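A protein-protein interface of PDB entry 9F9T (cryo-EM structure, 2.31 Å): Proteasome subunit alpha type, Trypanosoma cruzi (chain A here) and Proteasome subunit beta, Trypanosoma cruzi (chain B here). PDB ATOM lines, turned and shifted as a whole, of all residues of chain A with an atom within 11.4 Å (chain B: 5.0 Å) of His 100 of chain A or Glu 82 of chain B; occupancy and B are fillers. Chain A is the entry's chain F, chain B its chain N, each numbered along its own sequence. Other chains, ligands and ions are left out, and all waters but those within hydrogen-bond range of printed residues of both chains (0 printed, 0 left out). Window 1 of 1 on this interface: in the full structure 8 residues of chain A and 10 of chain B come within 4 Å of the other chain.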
ATOM      1  N   ASP A  68     -19.315  -6.700 -22.973  1.00  0.00           N
ATOM      2  CA  ASP A  68     -20.105  -6.567 -24.192  1.00  0.00           C
ATOM      3  C   ASP A  68     -21.065  -5.409 -23.951  1.00  0.00           C
ATOM      4  O   ASP A  68     -21.024  -4.791 -22.902  1.00  0.00           O
ATOM      5  CB  ASP A  68     -20.855  -7.876 -24.541  1.00  0.00           C
ATOM      6  CG  ASP A  68     -21.037  -8.193 -26.050  1.00  0.00           C
ATOM      7  OD1 ASP A  68     -22.100  -8.754 -26.431  1.00  0.00           O
ATOM      8  OD2 ASP A  68     -20.105  -7.909 -26.858  1.00  0.00           O
ATOM      9  N   HIS A  70     -23.913  -5.337 -22.896  1.00  0.00           N
ATOM     10  CA  HIS A  70     -24.803  -5.510 -21.769  1.00  0.00           C
ATOM     11  C   HIS A  70     -24.156  -6.068 -20.497  1.00  0.00           C
ATOM     12  O   HIS A  70     -24.898  -6.571 -19.612  1.00  0.00           O
ATOM     13  CB  HIS A  70     -25.913  -6.487 -22.130  1.00  0.00           C
ATOM     14  CG  HIS A  70     -25.484  -7.869 -22.377  1.00  0.00           C
ATOM     15  ND1 HIS A  70     -24.572  -8.171 -23.358  1.00  0.00           N
ATOM     16  CD2 HIS A  70     -25.848  -9.054 -21.833  1.00  0.00           C
ATOM     17  CE1 HIS A  70     -24.332  -9.496 -23.364  1.00  0.00           C
ATOM     18  NE2 HIS A  70     -25.111 -10.069 -22.446  1.00  0.00           N
ATOM     19  N   THR A  91     -14.695 -12.679 -25.819  1.00  0.00           N
ATOM     20  CA  THR A  91     -14.641 -13.537 -26.986  1.00  0.00           C
ATOM     21  C   THR A  91     -15.816 -14.502 -26.916  1.00  0.00           C
ATOM     22  O   THR A  91     -16.357 -14.858 -27.950  1.00  0.00           O
ATOM     23  CB  THR A  91     -13.318 -14.293 -26.988  1.00  0.00           C
ATOM     24  OG1 THR A  91     -12.264 -13.349 -27.224  1.00  0.00           O
ATOM     25  CG2 THR A  91     -13.363 -15.385 -28.016  1.00  0.00           C
ATOM     26  N   GLU A  92     -16.278 -14.825 -25.721  1.00  0.00           N
ATOM     27  CA  GLU A  92     -17.489 -15.626 -25.610  1.00  0.00           C
ATOM     28  C   GLU A  92     -18.749 -14.851 -25.987  1.00  0.00           C
ATOM     29  O   GLU A  92     -19.610 -15.427 -26.632  1.00  0.00           O
ATOM     30  CB  GLU A  92     -17.698 -16.214 -24.235  1.00  0.00           C
ATOM     31  CG  GLU A  92     -16.744 -17.359 -24.054  1.00  0.00           C
ATOM     32  CD  GLU A  92     -17.148 -18.690 -24.664  1.00  0.00           C
ATOM     33  OE1 GLU A  92     -18.262 -19.222 -24.312  1.00  0.00           O
ATOM     34  OE2 GLU A  92     -16.315 -19.235 -25.446  1.00  0.00           O
ATOM     35  N   CYS A  93     -18.843 -13.581 -25.618  1.00  0.00           N
ATOM     36  CA  CYS A  93     -20.031 -12.819 -25.907  1.00  0.00           C
ATOM     37  C   CYS A  93     -20.133 -12.476 -27.377  1.00  0.00           C
ATOM     38  O   CYS A  93     -21.227 -12.446 -27.940  1.00  0.00           O
ATOM     39  CB  CYS A  93     -20.003 -11.536 -25.131  1.00  0.00           C
ATOM     40  SG  CYS A  93     -20.198 -11.908 -23.375  1.00  0.00           S
ATOM     41  N   MET A  94     -19.012 -12.170 -27.979  1.00  0.00           N
ATOM     42  CA  MET A  94     -19.004 -11.885 -29.366  1.00  0.00           C
ATOM     43  C   MET A  94     -19.441 -13.134 -30.110  1.00  0.00           C
ATOM     44  O   MET A  94     -20.253 -13.061 -31.036  1.00  0.00           O
ATOM     45  CB  MET A  94     -17.596 -11.497 -29.829  1.00  0.00           C
ATOM     46  CG  MET A  94     -17.149 -10.005 -29.450  1.00  0.00           C
ATOM     47  SD  MET A  94     -15.444  -9.652 -30.115  1.00  0.00           S
ATOM     48  CE  MET A  94     -14.879  -8.366 -29.017  1.00  0.00           C
ATOM     49  N   ASN A  95     -18.874 -14.269 -29.762  1.00  0.00           N
ATOM     50  CA  ASN A  95     -19.231 -15.470 -30.448  1.00  0.00           C
ATOM     51  C   ASN A  95     -20.730 -15.642 -30.370  1.00  0.00           C
ATOM     52  O   ASN A  95     -21.387 -15.906 -31.397  1.00  0.00           O
ATOM     53  CB  ASN A  95     -18.558 -16.700 -29.863  1.00  0.00           C
ATOM     54  CG  ASN A  95     -17.110 -16.777 -30.285  1.00  0.00           C
ATOM     55  OD1 ASN A  95     -16.707 -16.116 -31.249  1.00  0.00           O
ATOM     56  ND2 ASN A  95     -16.313 -17.513 -29.506  1.00  0.00           N
ATOM     57  N   TYR A  96     -21.234 -15.532 -29.150  1.00  0.00           N
ATOM     58  CA  TYR A  96     -22.632 -15.739 -28.976  1.00  0.00           C
ATOM     59  C   TYR A  96     -23.438 -14.809 -29.899  1.00  0.00           C
ATOM     60  O   TYR A  96     -24.481 -15.218 -30.499  1.00  0.00           O
ATOM     61  CB  TYR A  96     -23.036 -15.567 -27.541  1.00  0.00           C
ATOM     62  CG  TYR A  96     -24.463 -16.076 -27.334  1.00  0.00           C
ATOM     63  CD1 TYR A  96     -24.742 -17.383 -26.892  1.00  0.00           C
ATOM     64  CD2 TYR A  96     -25.551 -15.192 -27.463  1.00  0.00           C
ATOM     65  CE1 TYR A  96     -26.034 -17.791 -26.551  1.00  0.00           C
ATOM     66  CE2 TYR A  96     -26.830 -15.580 -27.099  1.00  0.00           C
ATOM     67  CZ  TYR A  96     -27.081 -16.886 -26.682  1.00  0.00           C
ATOM     68  OH  TYR A  96     -28.406 -17.148 -26.520  1.00  0.00           O
ATOM     69  N   ARG A  97     -23.020 -13.539 -30.030  1.00  0.00           N
ATOM     70  CA  ARG A  97     -23.892 -12.592 -30.716  1.00  0.00           C
ATOM     71  C   ARG A  97     -23.746 -12.814 -32.207  1.00  0.00           C
ATOM     72  O   ARG A  97     -24.627 -12.550 -32.976  1.00  0.00           O
ATOM     73  CB  ARG A  97     -23.603 -11.161 -30.236  1.00  0.00           C
ATOM     74  CG  ARG A  97     -24.325 -10.088 -31.045  1.00  0.00           C
ATOM     75  CD  ARG A  97     -24.122  -8.647 -30.609  1.00  0.00           C
ATOM     76  NE  ARG A  97     -23.882  -8.551 -29.194  1.00  0.00           N
ATOM     77  CZ  ARG A  97     -24.838  -8.228 -28.368  1.00  0.00           C
ATOM     78  NH1 ARG A  97     -26.048  -8.064 -28.885  1.00  0.00           N
ATOM     79  NH2 ARG A  97     -24.629  -8.128 -27.062  1.00  0.00           N
ATOM     80  N   TYR A  98     -22.624 -13.352 -32.613  1.00  0.00           N
ATOM     81  CA  TYR A  98     -22.467 -13.734 -33.999  1.00  0.00           C
ATOM     82  C   TYR A  98     -23.420 -14.911 -34.270  1.00  0.00           C
ATOM     83  O   TYR A  98     -24.023 -14.978 -35.349  1.00  0.00           O
ATOM     84  CB  TYR A  98     -21.008 -14.058 -34.242  1.00  0.00           C
ATOM     85  CG  TYR A  98     -20.726 -14.678 -35.579  1.00  0.00           C
ATOM     86  CD1 TYR A  98     -20.624 -13.889 -36.686  1.00  0.00           C
ATOM     87  CD2 TYR A  98     -20.586 -16.035 -35.745  1.00  0.00           C
ATOM     88  CE1 TYR A  98     -20.420 -14.422 -37.936  1.00  0.00           C
ATOM     89  CE2 TYR A  98     -20.332 -16.591 -36.993  1.00  0.00           C
ATOM     90  CZ  TYR A  98     -20.303 -15.783 -38.113  1.00  0.00           C
ATOM     91  OH  TYR A  98     -20.051 -16.223 -39.397  1.00  0.00           O
ATOM     92  N   MET A  99     -23.586 -15.826 -33.320  1.00  0.00           N
ATOM     93  CA  MET A  99     -24.341 -16.995 -33.690  1.00  0.00           C
ATOM     94  C   MET A  99     -25.831 -16.668 -33.605  1.00  0.00           C
ATOM     95  O   MET A  99     -26.554 -17.037 -34.513  1.00  0.00           O
ATOM     96  CB  MET A  99     -23.952 -18.231 -32.886  1.00  0.00           C
ATOM     97  CG  MET A  99     -22.556 -18.787 -33.277  1.00  0.00           C
ATOM     98  SD  MET A  99     -22.305 -19.306 -35.073  1.00  0.00           S
ATOM     99  CE  MET A  99     -23.507 -20.618 -35.082  1.00  0.00           C
ATOM    100  N   HIS A 100     -26.230 -15.754 -32.716  1.00  0.00           N
ATOM    101  CA  HIS A 100     -27.622 -15.674 -32.303  1.00  0.00           C
ATOM    102  C   HIS A 100     -28.205 -14.313 -32.636  1.00  0.00           C
ATOM    103  O   HIS A 100     -29.401 -14.193 -32.681  1.00  0.00           O
ATOM    104  CB  HIS A 100     -27.806 -15.940 -30.780  1.00  0.00           C
ATOM    105  CG  HIS A 100     -27.329 -17.266 -30.341  1.00  0.00           C
ATOM    106  ND1 HIS A 100     -26.038 -17.541 -29.975  1.00  0.00           N
ATOM    107  CD2 HIS A 100     -27.966 -18.462 -30.404  1.00  0.00           C
ATOM    108  CE1 HIS A 100     -25.965 -18.842 -29.663  1.00  0.00           C
ATOM    109  NE2 HIS A 100     -27.155 -19.430 -29.878  1.00  0.00           N
ATOM    110  N   ASP A 101     -27.386 -13.281 -32.766  1.00  0.00           N
ATOM    111  CA  ASP A 101     -27.872 -11.908 -32.926  1.00  0.00           C
ATOM    112  C   ASP A 101     -28.574 -11.431 -31.660  1.00  0.00           C
ATOM    113  O   ASP A 101     -29.448 -10.606 -31.727  1.00  0.00           O
ATOM    114  CB  ASP A 101     -28.780 -11.786 -34.160  1.00  0.00           C
ATOM    115  CG  ASP A 101     -29.074 -10.384 -34.684  1.00  0.00           C
ATOM    116  OD1 ASP A 101     -28.194  -9.485 -34.557  1.00  0.00           O
ATOM    117  OD2 ASP A 101     -30.189 -10.206 -35.276  1.00  0.00           O
ATOM    118  N   SER A 102     -28.195 -11.924 -30.495  1.00  0.00           N
ATOM    119  CA  SER A 102     -28.781 -11.405 -29.282  1.00  0.00           C
ATOM    120  C   SER A 102     -27.704 -11.465 -28.232  1.00  0.00           C
ATOM    121  O   SER A 102     -26.593 -11.747 -28.611  1.00  0.00           O
ATOM    122  CB  SER A 102     -30.050 -12.132 -28.840  1.00  0.00           C
ATOM    123  OG  SER A 102     -29.702 -13.401 -28.335  1.00  0.00           O
ATOM    124  N   ASP A 103     -28.022 -11.141 -26.981  1.00  0.00           N
ATOM    125  CA  ASP A 103     -27.023 -11.005 -25.960  1.00  0.00           C
ATOM    126  C   ASP A 103     -26.717 -12.343 -25.307  1.00  0.00           C
ATOM    127  O   ASP A 103     -27.624 -12.964 -24.773  1.00  0.00           O
ATOM    128  CB  ASP A 103     -27.523 -10.105 -24.827  1.00  0.00           C
ATOM    129  CG  ASP A 103     -27.756  -8.626 -25.126  1.00  0.00           C
ATOM    130  OD1 ASP A 103     -26.948  -8.022 -25.946  1.00  0.00           O
ATOM    131  OD2 ASP A 103     -28.704  -8.034 -24.473  1.00  0.00           O
ATOM    132  N   ASN A 104     -25.426 -12.653 -25.119  1.00  0.00           N
ATOM    133  CA  ASN A 104     -25.051 -13.744 -24.219  1.00  0.00           C
ATOM    134  C   ASN A 104     -25.794 -13.619 -22.887  1.00  0.00           C
ATOM    135  O   ASN A 104     -25.661 -12.635 -22.170  1.00  0.00           O
ATOM    136  CB  ASN A 104     -23.551 -13.772 -23.927  1.00  0.00           C
ATOM    137  CG  ASN A 104     -22.938 -15.134 -23.663  1.00  0.00           C
ATOM    138  OD1 ASN A 104     -21.760 -15.343 -23.883  1.00  0.00           O
ATOM    139  ND2 ASN A 104     -23.736 -16.113 -23.345  1.00  0.00           N
ATOM    140  N   PRO A 105     -26.699 -14.566 -22.566  1.00  0.00           N
ATOM    141  CA  PRO A 105     -27.400 -14.554 -21.277  1.00  0.00           C
ATOM    142  C   PRO A 105     -26.448 -14.591 -20.103  1.00  0.00           C
ATOM    143  O   PRO A 105     -25.400 -15.227 -20.194  1.00  0.00           O
ATOM    144  CB  PRO A 105     -28.185 -15.855 -21.254  1.00  0.00           C
ATOM    145  CG  PRO A 105     -28.341 -16.228 -22.715  1.00  0.00           C
ATOM    146  CD  PRO A 105     -27.170 -15.628 -23.461  1.00  0.00           C
ATOM    147  N   LEU A 106     -26.805 -13.937 -18.999  1.00  0.00           N
ATOM    148  CA  LEU A 106     -25.804 -13.747 -17.965  1.00  0.00           C
ATOM    149  C   LEU A 106     -25.567 -15.031 -17.182  1.00  0.00           C
ATOM    150  O   LEU A 106     -24.447 -15.397 -16.946  1.00  0.00           O
ATOM    151  CB  LEU A 106     -26.198 -12.589 -17.059  1.00  0.00           C
ATOM    152  CG  LEU A 106     -25.582 -11.211 -17.344  1.00  0.00           C
ATOM    153  CD1 LEU A 106     -24.169 -11.116 -16.829  1.00  0.00           C
ATOM    154  CD2 LEU A 106     -25.631 -10.804 -18.820  1.00  0.00           C
ATOM    155  N   LEU A 108     -25.243 -17.937 -18.230  1.00  0.00           N
ATOM    156  CA  LEU A 108     -24.265 -18.693 -18.996  1.00  0.00           C
ATOM    157  C   LEU A 108     -22.854 -18.070 -18.931  1.00  0.00           C
ATOM    158  O   LEU A 108     -21.863 -18.766 -19.099  1.00  0.00           O
ATOM    159  CB  LEU A 108     -24.704 -18.788 -20.458  1.00  0.00           C
ATOM    160  CG  LEU A 108     -25.951 -19.636 -20.790  1.00  0.00           C
ATOM    161  CD1 LEU A 108     -25.994 -19.915 -22.290  1.00  0.00           C
ATOM    162  CD2 LEU A 108     -26.063 -20.962 -20.030  1.00  0.00           C
ATOM    163  N   ILE A 109     -22.733 -16.755 -18.795  1.00  0.00           N
ATOM    164  CA  ILE A 109     -21.430 -16.154 -18.611  1.00  0.00           C
ATOM    165  C   ILE A 109     -20.838 -16.647 -17.289  1.00  0.00           C
ATOM    166  O   ILE A 109     -19.765 -17.208 -17.267  1.00  0.00           O
ATOM    167  CB  ILE A 109     -21.523 -14.623 -18.678  1.00  0.00           C
ATOM    168  CG1 ILE A 109     -21.815 -14.213 -20.114  1.00  0.00           C
ATOM    169  CG2 ILE A 109     -20.225 -13.978 -18.180  1.00  0.00           C
ATOM    170  CD1 ILE A 109     -22.334 -12.827 -20.264  1.00  0.00           C
ATOM    171  N   ASP A 139     -30.051  -8.550 -19.021  1.00  0.00           N
ATOM    172  CA  ASP A 139     -30.513  -9.302 -20.188  1.00  0.00           C
ATOM    173  C   ASP A 139     -32.033  -9.451 -20.084  1.00  0.00           C
ATOM    174  O   ASP A 139     -32.674  -8.709 -19.337  1.00  0.00           O
ATOM    175  CB  ASP A 139     -29.789 -10.658 -20.322  1.00  0.00           C
ATOM    176  CG  ASP A 139     -30.122 -11.614 -19.181  1.00  0.00           C
ATOM    177  OD1 ASP A 139     -30.929 -11.205 -18.300  1.00  0.00           O
ATOM    178  OD2 ASP A 139     -29.553 -12.749 -19.130  1.00  0.00           O
ATOM    179  N   SER A 140     -32.601 -10.444 -20.786  1.00  0.00           N
ATOM    180  CA  SER A 140     -34.051 -10.603 -20.908  1.00  0.00           C
ATOM    181  C   SER A 140     -34.706 -10.998 -19.583  1.00  0.00           C
ATOM    182  O   SER A 140     -35.916 -10.865 -19.467  1.00  0.00           O
ATOM    183  CB  SER A 140     -34.448 -11.562 -22.040  1.00  0.00           C
ATOM    184  OG  SER A 140     -33.622 -12.718 -22.044  1.00  0.00           O
ATOM    185  N   THR A 141     -33.918 -11.433 -18.592  1.00  0.00           N
ATOM    186  CA  THR A 141     -34.440 -11.782 -17.277  1.00  0.00           C
ATOM    187  C   THR A 141     -34.026 -10.782 -16.190  1.00  0.00           C
ATOM    188  O   THR A 141     -34.087 -11.095 -15.000  1.00  0.00           O
ATOM    189  CB  THR A 141     -34.019 -13.205 -16.913  1.00  0.00           C
ATOM    190  OG1 THR A 141     -32.593 -13.330 -16.917  1.00  0.00           O
ATOM    191  CG2 THR A 141     -34.627 -14.204 -17.884  1.00  0.00           C
ATOM    192  N   HIS B  66     -29.193 -27.836 -29.915  1.00  0.00           N
ATOM    193  CA  HIS B  66     -28.771 -26.563 -29.339  1.00  0.00           C
ATOM    194  C   HIS B  66     -29.945 -25.917 -28.636  1.00  0.00           C
ATOM    195  O   HIS B  66     -29.954 -25.762 -27.442  1.00  0.00           O
ATOM    196  CB  HIS B  66     -28.080 -25.771 -30.457  1.00  0.00           C
ATOM    197  CG  HIS B  66     -27.713 -24.421 -30.015  1.00  0.00           C
ATOM    198  ND1 HIS B  66     -26.725 -24.152 -29.107  1.00  0.00           N
ATOM    199  CD2 HIS B  66     -28.291 -23.225 -30.286  1.00  0.00           C
ATOM    200  CE1 HIS B  66     -26.729 -22.848 -28.874  1.00  0.00           C
ATOM    201  NE2 HIS B  66     -27.681 -22.248 -29.543  1.00  0.00           N
ATOM    202  N   GLN B  70     -29.846 -25.618 -24.552  1.00  0.00           N
ATOM    203  CA  GLN B  70     -29.751 -24.278 -24.018  1.00  0.00           C
ATOM    204  C   GLN B  70     -30.847 -24.009 -23.013  1.00  0.00           C
ATOM    205  O   GLN B  70     -30.597 -23.412 -22.012  1.00  0.00           O
ATOM    206  CB  GLN B  70     -29.774 -23.278 -25.181  1.00  0.00           C
ATOM    207  CG  GLN B  70     -29.677 -21.835 -24.697  1.00  0.00           C
ATOM    208  CD  GLN B  70     -28.724 -20.916 -25.417  1.00  0.00           C
ATOM    209  OE1 GLN B  70     -27.552 -21.274 -25.661  1.00  0.00           O
ATOM    210  NE2 GLN B  70     -29.224 -19.700 -25.601  1.00  0.00           N
ATOM    211  N   ALA B  77     -35.209 -19.939 -23.642  1.00  0.00           N
ATOM    212  CA  ALA B  77     -35.814 -20.542 -24.822  1.00  0.00           C
ATOM    213  C   ALA B  77     -35.520 -19.662 -26.006  1.00  0.00           C
ATOM    214  O   ALA B  77     -36.003 -18.544 -26.062  1.00  0.00           O
ATOM    215  CB  ALA B  77     -37.321 -20.627 -24.651  1.00  0.00           C
ATOM    216  N   LEU B  78     -34.753 -20.172 -26.950  1.00  0.00           N
ATOM    217  CA  LEU B  78     -34.448 -19.393 -28.108  1.00  0.00           C
ATOM    218  C   LEU B  78     -35.700 -19.073 -28.934  1.00  0.00           C
ATOM    219  O   LEU B  78     -36.554 -19.942 -29.143  1.00  0.00           O
ATOM    220  CB  LEU B  78     -33.524 -20.261 -28.922  1.00  0.00           C
ATOM    221  CG  LEU B  78     -32.083 -20.368 -28.465  1.00  0.00           C
ATOM    222  CD1 LEU B  78     -31.210 -20.763 -29.666  1.00  0.00           C
ATOM    223  CD2 LEU B  78     -31.626 -19.031 -27.860  1.00  0.00           C
ATOM    224  N   THR B  79     -35.680 -17.853 -29.493  1.00  0.00           N
ATOM    225  CA  THR B  79     -36.699 -17.260 -30.302  1.00  0.00           C
ATOM    226  C   THR B  79     -36.511 -17.539 -31.783  1.00  0.00           C
ATOM    227  O   THR B  79     -35.502 -18.078 -32.209  1.00  0.00           O
ATOM    228  CB  THR B  79     -36.683 -15.737 -30.192  1.00  0.00           C
ATOM    229  OG1 THR B  79     -35.549 -15.216 -30.877  1.00  0.00           O
ATOM    230  CG2 THR B  79     -36.750 -15.272 -28.760  1.00  0.00           C
ATOM    231  N   PRO B  80     -37.531 -17.297 -32.624  1.00  0.00           N
ATOM    232  CA  PRO B  80     -37.405 -17.526 -34.037  1.00  0.00           C
ATOM    233  C   PRO B  80     -36.243 -16.787 -34.612  1.00  0.00           C
ATOM    234  O   PRO B  80     -35.579 -17.307 -35.450  1.00  0.00           O
ATOM    235  CB  PRO B  80     -38.717 -17.015 -34.643  1.00  0.00           C
ATOM    236  CG  PRO B  80     -39.705 -17.171 -33.520  1.00  0.00           C
ATOM    237  CD  PRO B  80     -38.908 -16.953 -32.270  1.00  0.00           C
ATOM    238  N   ASN B  81     -36.046 -15.575 -34.197  1.00  0.00           N
ATOM    239  CA  ASN B  81     -35.032 -14.727 -34.782  1.00  0.00           C
ATOM    240  C   ASN B  81     -33.632 -15.290 -34.488  1.00  0.00           C
ATOM    241  O   ASN B  81     -32.767 -15.291 -35.369  1.00  0.00           O
ATOM    242  CB  ASN B  81     -35.278 -13.278 -34.330  1.00  0.00           C
ATOM    243  CG  ASN B  81     -34.767 -12.370 -35.425  1.00  0.00           C
ATOM    244  OD1 ASN B  81     -35.511 -12.050 -36.366  1.00  0.00           O
ATOM    245  ND2 ASN B  81     -33.463 -12.052 -35.392  1.00  0.00           N
ATOM    246  N   GLU B  82     -33.467 -15.820 -33.284  1.00  0.00           N
ATOM    247  CA  GLU B  82     -32.211 -16.385 -32.867  1.00  0.00           C
ATOM    248  C   GLU B  82     -31.936 -17.694 -33.585  1.00  0.00           C
ATOM    249  O   GLU B  82     -30.813 -17.921 -34.058  1.00  0.00           O
ATOM    250  CB  GLU B  82     -32.200 -16.616 -31.361  1.00  0.00           C
ATOM    251  CG  GLU B  82     -32.283 -15.360 -30.499  1.00  0.00           C
ATOM    252  CD  GLU B  82     -32.660 -15.553 -29.001  1.00  0.00           C
ATOM    253  OE1 GLU B  82     -33.575 -16.397 -28.622  1.00  0.00           O
ATOM    254  OE2 GLU B  82     -32.104 -14.780 -28.138  1.00  0.00           O
ATOM    255  N   VAL B  83     -32.958 -18.533 -33.719  1.00  0.00           N
ATOM    256  CA  VAL B  83     -32.867 -19.814 -34.412  1.00  0.00           C
ATOM    257  C   VAL B  83     -32.476 -19.570 -35.841  1.00  0.00           C
ATOM    258  O   VAL B  83     -31.634 -20.241 -36.396  1.00  0.00           O
ATOM    259  CB  VAL B  83     -34.220 -20.552 -34.320  1.00  0.00           C
ATOM    260  CG1 VAL B  83     -34.375 -21.703 -35.304  1.00  0.00           C
ATOM    261  CG2 VAL B  83     -34.472 -21.022 -32.908  1.00  0.00           C
ATOM    262  N   PHE B  84     -33.100 -18.579 -36.412  1.00  0.00           N
ATOM    263  CA  PHE B  84     -32.847 -18.229 -37.789  1.00  0.00           C
ATOM    264  C   PHE B  84     -31.418 -17.779 -38.018  1.00  0.00           C
ATOM    265  O   PHE B  84     -30.733 -18.193 -38.908  1.00  0.00           O
ATOM    266  CB  PHE B  84     -33.831 -17.160 -38.161  1.00  0.00           C
ATOM    267  CG  PHE B  84     -33.786 -16.751 -39.609  1.00  0.00           C
ATOM    268  CD1 PHE B  84     -34.341 -17.590 -40.557  1.00  0.00           C
ATOM    269  CD2 PHE B  84     -33.265 -15.505 -39.989  1.00  0.00           C
ATOM    270  CE1 PHE B  84     -34.363 -17.255 -41.876  1.00  0.00           C
ATOM    271  CE2 PHE B  84     -33.266 -15.171 -41.317  1.00  0.00           C
ATOM    272  CZ  PHE B  84     -33.855 -16.015 -42.255  1.00  0.00           C
ATOM    273  N   CYS B  85     -30.977 -16.856 -37.231  1.00  0.00           N
ATOM    274  CA  CYS B  85     -29.578 -16.470 -37.225  1.00  0.00           C
ATOM    275  C   CYS B  85     -28.616 -17.653 -37.094  1.00  0.00           C
ATOM    276  O   CYS B  85     -27.727 -17.770 -37.899  1.00  0.00           O
ATOM    277  CB  CYS B  85     -29.343 -15.448 -36.134  1.00  0.00           C
ATOM    278  SG  CYS B  85     -27.700 -14.781 -36.385  1.00  0.00           S
ATOM    279  N   TYR B  86     -28.819 -18.569 -36.194  1.00  0.00           N
ATOM    280  CA  TYR B  86     -27.923 -19.689 -36.036  1.00  0.00           C
ATOM    281  C   TYR B  86     -27.913 -20.625 -37.235  1.00  0.00           C
ATOM    282  O   TYR B  86     -26.891 -21.090 -37.678  1.00  0.00           O
ATOM    283  CB  TYR B  86     -28.492 -20.328 -34.763  1.00  0.00           C
ATOM    284  CG  TYR B  86     -27.637 -21.404 -34.148  1.00  0.00           C
ATOM    285  CD1 TYR B  86     -26.614 -21.123 -33.255  1.00  0.00           C
ATOM    286  CD2 TYR B  86     -27.804 -22.722 -34.511  1.00  0.00           C
ATOM    287  CE1 TYR B  86     -25.823 -22.116 -32.699  1.00  0.00           C
ATOM    288  CE2 TYR B  86     -26.997 -23.728 -33.991  1.00  0.00           C
ATOM    289  CZ  TYR B  86     -26.011 -23.433 -33.078  1.00  0.00           C
ATOM    290  OH  TYR B  86     -25.267 -24.488 -32.611  1.00  0.00           O
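A ring nitrogen (NE2) of His 66 of chain B lies within hydrogen-bond range of a ring nitrogen (NE2) of His 100 of chain A (2.9 Å).
OH of Tyr 96 of chain A sits at hydrogen-bond distance from NE2 of Gln 70 of chain B (2.8 Å).
The side-chain carboxylate (OE2) of Glu 82 of chain B sits at hydrogen-bond distance from the side-chain hydroxyl (OG) of Ser 102 of chain A, at 2.8 Å.
SG of Cys 85 of chain B is in hydrogen-bond range of O of Met 99 of chain A, 3.1 Å away.
N of Tyr 86 of chain B is in hydrogen-bond range of O of Met 99 of chain A, 3.2 Å away.
Tyr 96 of chain A touches Leu 78 of chain B.
Tyr 98 of chain A touches Cys 85 of chain B (O to SG, 3.8 Å).
O of His 100 of chain A touches CA of Glu 82 of chain B, 3.6 Å away.
Cys 85 of chain B touches His 100 of chain A.
His 100 of chain A touches Tyr 86 of chain B.
Asp 101 of chain A touches Asn 81 of chain B (OD2 to ND2, 3.8 Å).
Asp 101 of chain A touches Cys 85 of chain B (CB to SG, 3.9 Å).
Leu 108 of chain A touches Gln 70 of chain B.
Met 94 of chain A touches none of the printed residues of chain B.
His 100 of chain A touches four residues of chain B.
Of the printed residues of chain B, Leu 108 of chain A touches Gln 70.
Printed residues of chain A within 4 Å of His 66 of chain B: His 100.
Ala 77 of chain B touches none of the printed residues of chain A.
Leu 78 of chain B touches just one residue of chain A: Tyr 96 (3.96 Å).
No residue of chain A comes within 4 Å of Thr 79 of chain B.
No residue of chain A comes within 4 Å of Pro 80 of chain B.
Of chain A, only His 100 (3.6 Å) and Ser 102 (2.8 Å) come within 4 Å of Glu 82 of chain B.
No residue of chain A comes within 4 Å of Val 83 of chain B.
Tyr 86 of chain B touches two residues of chain A.
The nearest residue of chain B that does not touch His 100 of chain A is Leu 78 of chain B (4.05 Å).
The nearest printed residue of chain B that does not touch Leu 108 of chain A is His 66 of chain B (7.2 Å).
Of the 12 printed residues of chain B, 7 touch a printed residue of chain A.
Among the printed residues, no Asp or Glu carboxylate lies within 4 Å of a Lys or Arg side-chain nitrogen of the other chain.
N of Asn 81 of chain B lies close to OG1 of Thr 79 of chain B (3.4 Å).
The side-chain carboxylate (OE1) of Glu 82 of chain B lies within hydrogen-bond range of the backbone NH (N) of Thr 79 of chain B (2.7 Å).
ND1 of His 100 of chain A is in hydrogen-bond range of O of Tyr 96 of chain A, 2.8 Å away.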
